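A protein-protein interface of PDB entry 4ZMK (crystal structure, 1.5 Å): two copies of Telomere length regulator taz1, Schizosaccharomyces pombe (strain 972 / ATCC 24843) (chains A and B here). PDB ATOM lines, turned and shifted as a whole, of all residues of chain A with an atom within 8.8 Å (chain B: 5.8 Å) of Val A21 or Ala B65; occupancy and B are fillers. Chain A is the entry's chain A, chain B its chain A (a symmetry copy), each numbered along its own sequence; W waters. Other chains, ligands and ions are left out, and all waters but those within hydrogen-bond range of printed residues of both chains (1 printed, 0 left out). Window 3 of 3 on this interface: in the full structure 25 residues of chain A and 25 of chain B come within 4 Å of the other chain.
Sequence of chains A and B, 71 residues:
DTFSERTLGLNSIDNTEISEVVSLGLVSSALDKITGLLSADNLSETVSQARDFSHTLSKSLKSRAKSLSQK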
ATOM      1  N   ILE A  18      19.155  15.170 -14.878  1.00  0.00           N
ATOM      2  CA  ILE A  18      19.550  14.799 -16.228  1.00  0.00           C
ATOM      3  C   ILE A  18      20.939  15.338 -16.506  1.00  0.00           C
ATOM      4  O   ILE A  18      21.173  16.533 -16.355  1.00  0.00           O
ATOM      5  CB  ILE A  18      18.568  15.347 -17.259  1.00  0.00           C
ATOM      6  CG1 ILE A  18      17.230  14.637 -17.122  1.00  0.00           C
ATOM      7  CG2 ILE A  18      19.096  15.161 -18.659  1.00  0.00           C
ATOM      8  CD1 ILE A  18      16.238  15.055 -18.152  1.00  0.00           C
ATOM      9  N   SER A  19      21.866  14.466 -16.893  1.00  0.00           N
ATOM     10  CA  SER A  19      23.244  14.884 -17.124  1.00  0.00           C
ATOM     11  C   SER A  19      23.380  15.703 -18.399  1.00  0.00           C
ATOM     12  O   SER A  19      22.491  15.695 -19.248  1.00  0.00           O
ATOM     13  CB  SER A  19      24.160  13.673 -17.206  1.00  0.00           C
ATOM     14  OG  SER A  19      23.964  12.993 -18.431  1.00  0.00           O
ATOM     15  N   GLU A  20      24.502  16.396 -18.545  1.00  0.00           N
ATOM     16  CA  GLU A  20      24.694  17.241 -19.713  1.00  0.00           C
ATOM     17  C   GLU A  20      24.657  16.436 -21.003  1.00  0.00           C
ATOM     18  O   GLU A  20      24.041  16.863 -21.967  1.00  0.00           O
ATOM     19  CB  GLU A  20      26.005  18.011 -19.626  1.00  0.00           C
ATOM     20  CG  GLU A  20      26.114  19.088 -20.688  1.00  0.00           C
ATOM     21  CD  GLU A  20      27.345  19.962 -20.526  1.00  0.00           C
ATOM     22  OE1 GLU A  20      28.186  19.654 -19.662  1.00  0.00           O
ATOM     23  OE2 GLU A  20      27.482  20.958 -21.268  1.00  0.00           O
ATOM     24  N   VAL A  21      25.300  15.271 -21.020  1.00  0.00           N
ATOM     25  CA  VAL A  21      25.354  14.458 -22.237  1.00  0.00           C
ATOM     26  C   VAL A  21      23.948  14.002 -22.637  1.00  0.00           C
ATOM     27  O   VAL A  21      23.584  14.062 -23.802  1.00  0.00           O
ATOM     28  CB  VAL A  21      26.309  13.226 -22.074  1.00  0.00           C
ATOM     29  CG1 VAL A  21      26.017  12.144 -23.108  1.00  0.00           C
ATOM     30  CG2 VAL A  21      27.756  13.662 -22.171  1.00  0.00           C
ATOM     31  N   VAL A  22      23.154  13.572 -21.669  1.00  0.00           N
ATOM     32  CA  VAL A  22      21.784  13.181 -21.958  1.00  0.00           C
ATOM     33  C   VAL A  22      20.992  14.379 -22.480  1.00  0.00           C
ATOM     34  O   VAL A  22      20.250  14.256 -23.444  1.00  0.00           O
ATOM     35  CB  VAL A  22      21.087  12.586 -20.719  1.00  0.00           C
ATOM     36  CG1 VAL A  22      19.613  12.313 -21.006  1.00  0.00           C
ATOM     37  CG2 VAL A  22      21.802  11.311 -20.281  1.00  0.00           C
ATOM     38  N   SER A  23      21.168  15.538 -21.853  1.00  0.00           N
ATOM     39  CA  SER A  23      20.545  16.777 -22.301  1.00  0.00           C
ATOM     40  C   SER A  23      20.908  17.076 -23.755  1.00  0.00           C
ATOM     41  O   SER A  23      20.060  17.415 -24.567  1.00  0.00           O
ATOM     42  CB  SER A  23      20.970  17.938 -21.393  1.00  0.00           C
ATOM     43  OG  SER A  23      20.526  19.183 -21.892  1.00  0.00           O
ATOM     44  N   LEU A  24      22.192  16.946 -24.075  1.00  0.00           N
ATOM     45  CA  LEU A  24      22.663  17.214 -25.433  1.00  0.00           C
ATOM     46  C   LEU A  24      22.047  16.237 -26.432  1.00  0.00           C
ATOM     47  O   LEU A  24      21.814  16.588 -27.573  1.00  0.00           O
ATOM     48  CB  LEU A  24      24.188  17.151 -25.503  1.00  0.00           C
ATOM     49  CG  LEU A  24      24.882  18.312 -24.791  1.00  0.00           C
ATOM     50  CD1 LEU A  24      26.402  18.151 -24.802  1.00  0.00           C
ATOM     51  CD2 LEU A  24      24.457  19.630 -25.421  1.00  0.00           C
ATOM     52  N   GLY A  25      21.769  15.017 -25.987  1.00  0.00           N
ATOM     53  CA  GLY A  25      21.074  14.047 -26.814  1.00  0.00           C
ATOM     54  C   GLY A  25      19.649  14.464 -27.117  1.00  0.00           C
ATOM     55  O   GLY A  25      19.160  14.236 -28.210  1.00  0.00           O
ATOM     56  N   LEU A  26      18.979  15.076 -26.145  1.00  0.00           N
ATOM     57  CA  LEU A  26      17.607  15.525 -26.330  1.00  0.00           C
ATOM     58  C   LEU A  26      17.552  16.742 -27.253  1.00  0.00           C
ATOM     59  O   LEU A  26      16.659  16.849 -28.086  1.00  0.00           O
ATOM     60  CB  LEU A  26      16.959  15.848 -24.976  1.00  0.00           C
ATOM     61  CG  LEU A  26      16.733  14.670 -24.023  1.00  0.00           C
ATOM     62  CD1 LEU A  26      16.193  15.148 -22.695  1.00  0.00           C
ATOM     63  CD2 LEU A  26      15.802  13.663 -24.633  1.00  0.00           C
ATOM     64  N   VAL A  27      18.515  17.651 -27.110  1.00  0.00           N
ATOM     65  CA  VAL A  27      18.566  18.852 -27.940  1.00  0.00           C
ATOM     66  C   VAL A  27      18.890  18.489 -29.387  1.00  0.00           C
ATOM     67  O   VAL A  27      18.208  18.929 -30.312  1.00  0.00           O
ATOM     68  CB  VAL A  27      19.587  19.852 -27.392  1.00  0.00           C
ATOM     69  CG1 VAL A  27      19.611  21.094 -28.237  1.00  0.00           C
ATOM     70  CG2 VAL A  27      19.228  20.199 -25.964  1.00  0.00           C
ATOM     71  N   SER A  28      19.924  17.675 -29.567  1.00  0.00           N
ATOM     72  CA  SER A  28      20.308  17.158 -30.875  1.00  0.00           C
ATOM     73  C   SER A  28      19.117  16.546 -31.609  1.00  0.00           C
ATOM     74  O   SER A  28      18.891  16.813 -32.780  1.00  0.00           O
ATOM     75  CB  SER A  28      21.419  16.112 -30.712  1.00  0.00           C
ATOM     76  OG  SER A  28      21.867  15.611 -31.957  1.00  0.00           O
ATOM     77  N   ARG A  64      16.217  25.191 -18.236  1.00  0.00           N
ATOM     78  CA  ARG A  64      17.241  24.288 -17.733  1.00  0.00           C
ATOM     79  C   ARG A  64      18.422  25.070 -17.162  1.00  0.00           C
ATOM     80  O   ARG A  64      18.890  24.780 -16.073  1.00  0.00           O
ATOM     81  CB  ARG A  64      17.712  23.335 -18.832  1.00  0.00           C
ATOM     82  CG  ARG A  64      18.889  22.477 -18.410  1.00  0.00           C
ATOM     83  CD  ARG A  64      19.284  21.457 -19.456  1.00  0.00           C
ATOM     84  NE  ARG A  64      20.410  20.679 -18.970  1.00  0.00           N
ATOM     85  CZ  ARG A  64      20.292  19.639 -18.154  1.00  0.00           C
ATOM     86  NH1 ARG A  64      19.090  19.237 -17.752  1.00  0.00           N
ATOM     87  NH2 ARG A  64      21.376  19.002 -17.742  1.00  0.00           N
ATOM     88  N   SER B  60      27.344  20.453 -33.874  1.00  0.00           N
ATOM     89  CA  SER B  60      28.280  20.971 -32.887  1.00  0.00           C
ATOM     90  C   SER B  60      27.965  20.436 -31.492  1.00  0.00           C
ATOM     91  O   SER B  60      28.871  20.247 -30.681  1.00  0.00           O
ATOM     92  CB  SER B  60      28.284  22.501 -32.884  1.00  0.00           C
ATOM     93  OG  SER B  60      27.237  23.024 -32.092  1.00  0.00           O
ATOM     94  N   LEU B  61      26.695  20.166 -31.222  1.00  0.00           N
ATOM     95  CA  LEU B  61      26.308  19.614 -29.924  1.00  0.00           C
ATOM     96  C   LEU B  61      26.683  18.126 -29.822  1.00  0.00           C
ATOM     97  O   LEU B  61      27.016  17.621 -28.751  1.00  0.00           O
ATOM     98  CB  LEU B  61      24.813  19.840 -29.684  1.00  0.00           C
ATOM     99  CG  LEU B  61      24.451  21.328 -29.540  1.00  0.00           C
ATOM    100  CD1 LEU B  61      23.041  21.508 -29.063  1.00  0.00           C
ATOM    101  CD2 LEU B  61      25.418  22.001 -28.572  1.00  0.00           C
ATOM    102  N   LYS B  62      26.645  17.429 -30.947  1.00  0.00           N
ATOM    103  CA  LYS B  62      27.119  16.053 -31.002  1.00  0.00           C
ATOM    104  C   LYS B  62      28.621  16.026 -30.732  1.00  0.00           C
ATOM    105  O   LYS B  62      29.119  15.157 -30.021  1.00  0.00           O
ATOM    106  CB  LYS B  62      26.799  15.420 -32.359  1.00  0.00           C
ATOM    107  CG  LYS B  62      25.308  15.276 -32.644  1.00  0.00           C
ATOM    108  CD  LYS B  62      25.055  14.763 -34.061  1.00  0.00           C
ATOM    109  CE  LYS B  62      23.565  14.735 -34.381  1.00  0.00           C
ATOM    110  NZ  LYS B  62      23.260  14.291 -35.769  1.00  0.00           N
ATOM    111  N   SER B  63      29.335  16.993 -31.299  1.00  0.00           N
ATOM    112  CA  SER B  63      30.768  17.112 -31.079  1.00  0.00           C
ATOM    113  C   SER B  63      31.053  17.433 -29.614  1.00  0.00           C
ATOM    114  O   SER B  63      31.962  16.871 -29.010  1.00  0.00           O
ATOM    115  CB  SER B  63      31.363  18.186 -31.986  1.00  0.00           C
ATOM    116  OG  SER B  63      32.772  18.253 -31.853  1.00  0.00           O
ATOM    117  N   ARG B  64      30.269  18.339 -29.044  1.00  0.00           N
ATOM    118  CA  ARG B  64      30.437  18.676 -27.638  1.00  0.00           C
ATOM    119  C   ARG B  64      30.166  17.462 -26.753  1.00  0.00           C
ATOM    120  O   ARG B  64      30.938  17.163 -25.856  1.00  0.00           O
ATOM    121  CB  ARG B  64      29.525  19.839 -27.246  1.00  0.00           C
ATOM    122  CG  ARG B  64      29.541  20.130 -25.758  1.00  0.00           C
ATOM    123  CD  ARG B  64      28.726  21.349 -25.384  1.00  0.00           C
ATOM    124  NE  ARG B  64      28.799  21.558 -23.949  1.00  0.00           N
ATOM    125  CZ  ARG B  64      29.806  22.176 -23.343  1.00  0.00           C
ATOM    126  NH1 ARG B  64      30.815  22.670 -24.055  1.00  0.00           N
ATOM    127  NH2 ARG B  64      29.801  22.300 -22.025  1.00  0.00           N
ATOM    128  N   ALA B  65      29.067  16.759 -27.016  1.00  0.00           N
ATOM    129  CA  ALA B  65      28.733  15.528 -26.287  1.00  0.00           C
ATOM    130  C   ALA B  65      29.863  14.510 -26.326  1.00  0.00           C
ATOM    131  O   ALA B  65      30.163  13.862 -25.324  1.00  0.00           O
ATOM    132  CB  ALA B  65      27.465  14.907 -26.844  1.00  0.00           C
ATOM    133  N   LYS B  66      30.485  14.362 -27.489  1.00  0.00           N
ATOM    134  CA  LYS B  66      31.646  13.494 -27.618  1.00  0.00           C
ATOM    135  C   LYS B  66      32.800  13.954 -26.708  1.00  0.00           C
ATOM    136  O   LYS B  66      33.315  13.174 -25.917  1.00  0.00           O
ATOM    137  CB  LYS B  66      32.115  13.437 -29.066  1.00  0.00           C
ATOM    138  CG  LYS B  66      33.330  12.555 -29.241  1.00  0.00           C
ATOM    139  CD  LYS B  66      33.844  12.528 -30.661  1.00  0.00           C
ATOM    140  CE  LYS B  66      34.882  11.421 -30.784  1.00  0.00           C
ATOM    141  NZ  LYS B  66      35.232  11.122 -32.183  1.00  0.00           N
ATOM    142  N   SER B  67      33.187  15.224 -26.817  1.00  0.00           N
ATOM    143  CA  SER B  67      34.252  15.780 -25.992  1.00  0.00           C
ATOM    144  C   SER B  67      33.976  15.621 -24.514  1.00  0.00           C
ATOM    145  O   SER B  67      34.891  15.360 -23.739  1.00  0.00           O
ATOM    146  CB  SER B  67      34.465  17.256 -26.310  1.00  0.00           C
ATOM    147  OG  SER B  67      35.080  17.409 -27.572  1.00  0.00           O
ATOM    148  N   LEU B  68      32.716  15.774 -24.122  1.00  0.00           N
ATOM    149  CA  LEU B  68      32.354  15.690 -22.708  1.00  0.00           C
ATOM    150  C   LEU B  68      32.408  14.270 -22.197  1.00  0.00           C
ATOM    151  O   LEU B  68      32.834  14.024 -21.070  1.00  0.00           O
ATOM    152  CB  LEU B  68      30.961  16.257 -22.465  1.00  0.00           C
ATOM    153  CG  LEU B  68      30.866  17.778 -22.527  1.00  0.00           C
ATOM    154  CD1 LEU B  68      29.411  18.210 -22.457  1.00  0.00           C
ATOM    155  CD2 LEU B  68      31.704  18.431 -21.418  1.00  0.00           C
ATOM    156  N   SER B  69      31.974  13.334 -23.030  1.00  0.00           N
ATOM    157  CA  SER B  69      31.920  11.940 -22.624  1.00  0.00           C
ATOM    158  C   SER B  69      33.333  11.367 -22.500  1.00  0.00           C
ATOM    159  O   SER B  69      33.564  10.444 -21.727  1.00  0.00           O
ATOM    160  CB  SER B  69      31.083  11.120 -23.613  1.00  0.00           C
ATOM    161  OG  SER B  69      31.765  10.941 -24.839  1.00  0.00           O
ATOM    162  N   GLN B  70      34.275  11.928 -23.258  1.00  0.00           N
ATOM    163  CA  GLN B  70      35.681  11.538 -23.177  1.00  0.00           C
ATOM    164  C   GLN B  70      36.212  11.728 -21.758  1.00  0.00           C
ATOM    165  O   GLN B  70      37.105  11.013 -21.319  1.00  0.00           O
ATOM    166  CB  GLN B  70      36.526  12.357 -24.149  1.00  0.00           C
ATOM    167  CG  GLN B  70      37.351  11.536 -25.105  1.00  0.00           C
ATOM    168  CD  GLN B  70      36.589  11.184 -26.369  1.00  0.00           C
ATOM    169  OE1 GLN B  70      36.538  11.980 -27.309  1.00  0.00           O
ATOM    170  NE2 GLN B  70      35.991   9.988 -26.400  1.00  0.00           N
HETATM  171  O   HOH W   1      25.596  21.823 -22.873  1.00  0.00           O
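The side-chain carboxylate (OE2) of Glu A20 lies within salt-bridge range of the guanidinium group (NH2) of Arg B64.
O of Ala B65 sits close to OG of Ser B69, 3.4 Å away.
Among the printed residues, pairs that only touch across the chains: Glu A20 with Leu B68 (3.3 Å), Val A21 with Ala B65 (3.97 Å), Leu A24 with Arg B64 (3.8 Å), Leu A24 with Ala B65 (3.7 Å), Leu A24 with Leu B68 (3.8 Å), Val A27 with Leu B61 (3.6 Å) and Ser A28 with Lys B62 (3.1 Å).
Gly A25 touches none of the printed residues of chain B. Printed residues of chain A within 4 Å of Leu B61: Val A27. Printed residues of chain A within 4 Å of Lys B62: Ser A28. Of the printed residues of chain A, Ala B65 touches Val A21 and Leu A24. Ser B69 touches none of the printed residues of chain A. The nearest residue of chain A that does not touch Ala B65 is Gly A25 (5.8 Å).
Hydrophobic or aromatic side chains of chain B that line the printed part of chain A: Leu B61, Ala B65 and Leu B68. Of the 12 printed residues of chain A, 5 touch a printed residue of chain B. Hydrophobic or aromatic side chains of chain A within 4 Å of the printed part of chain B: Val A21, Leu A24 and Val A27. Among the printed residues, 8 pairs touch across the chains. Among the printed residues, Asp or Glu carboxylates within 4 Å of a Lys or Arg side-chain nitrogen of the other chain: Glu A20 with Arg B64 (2.8 Å).
1 position is printed for both chains.
Water W1 bridges the side-chain carboxylate (OE2) of Glu A20 and the guanidinium group (NE) of Arg B64.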
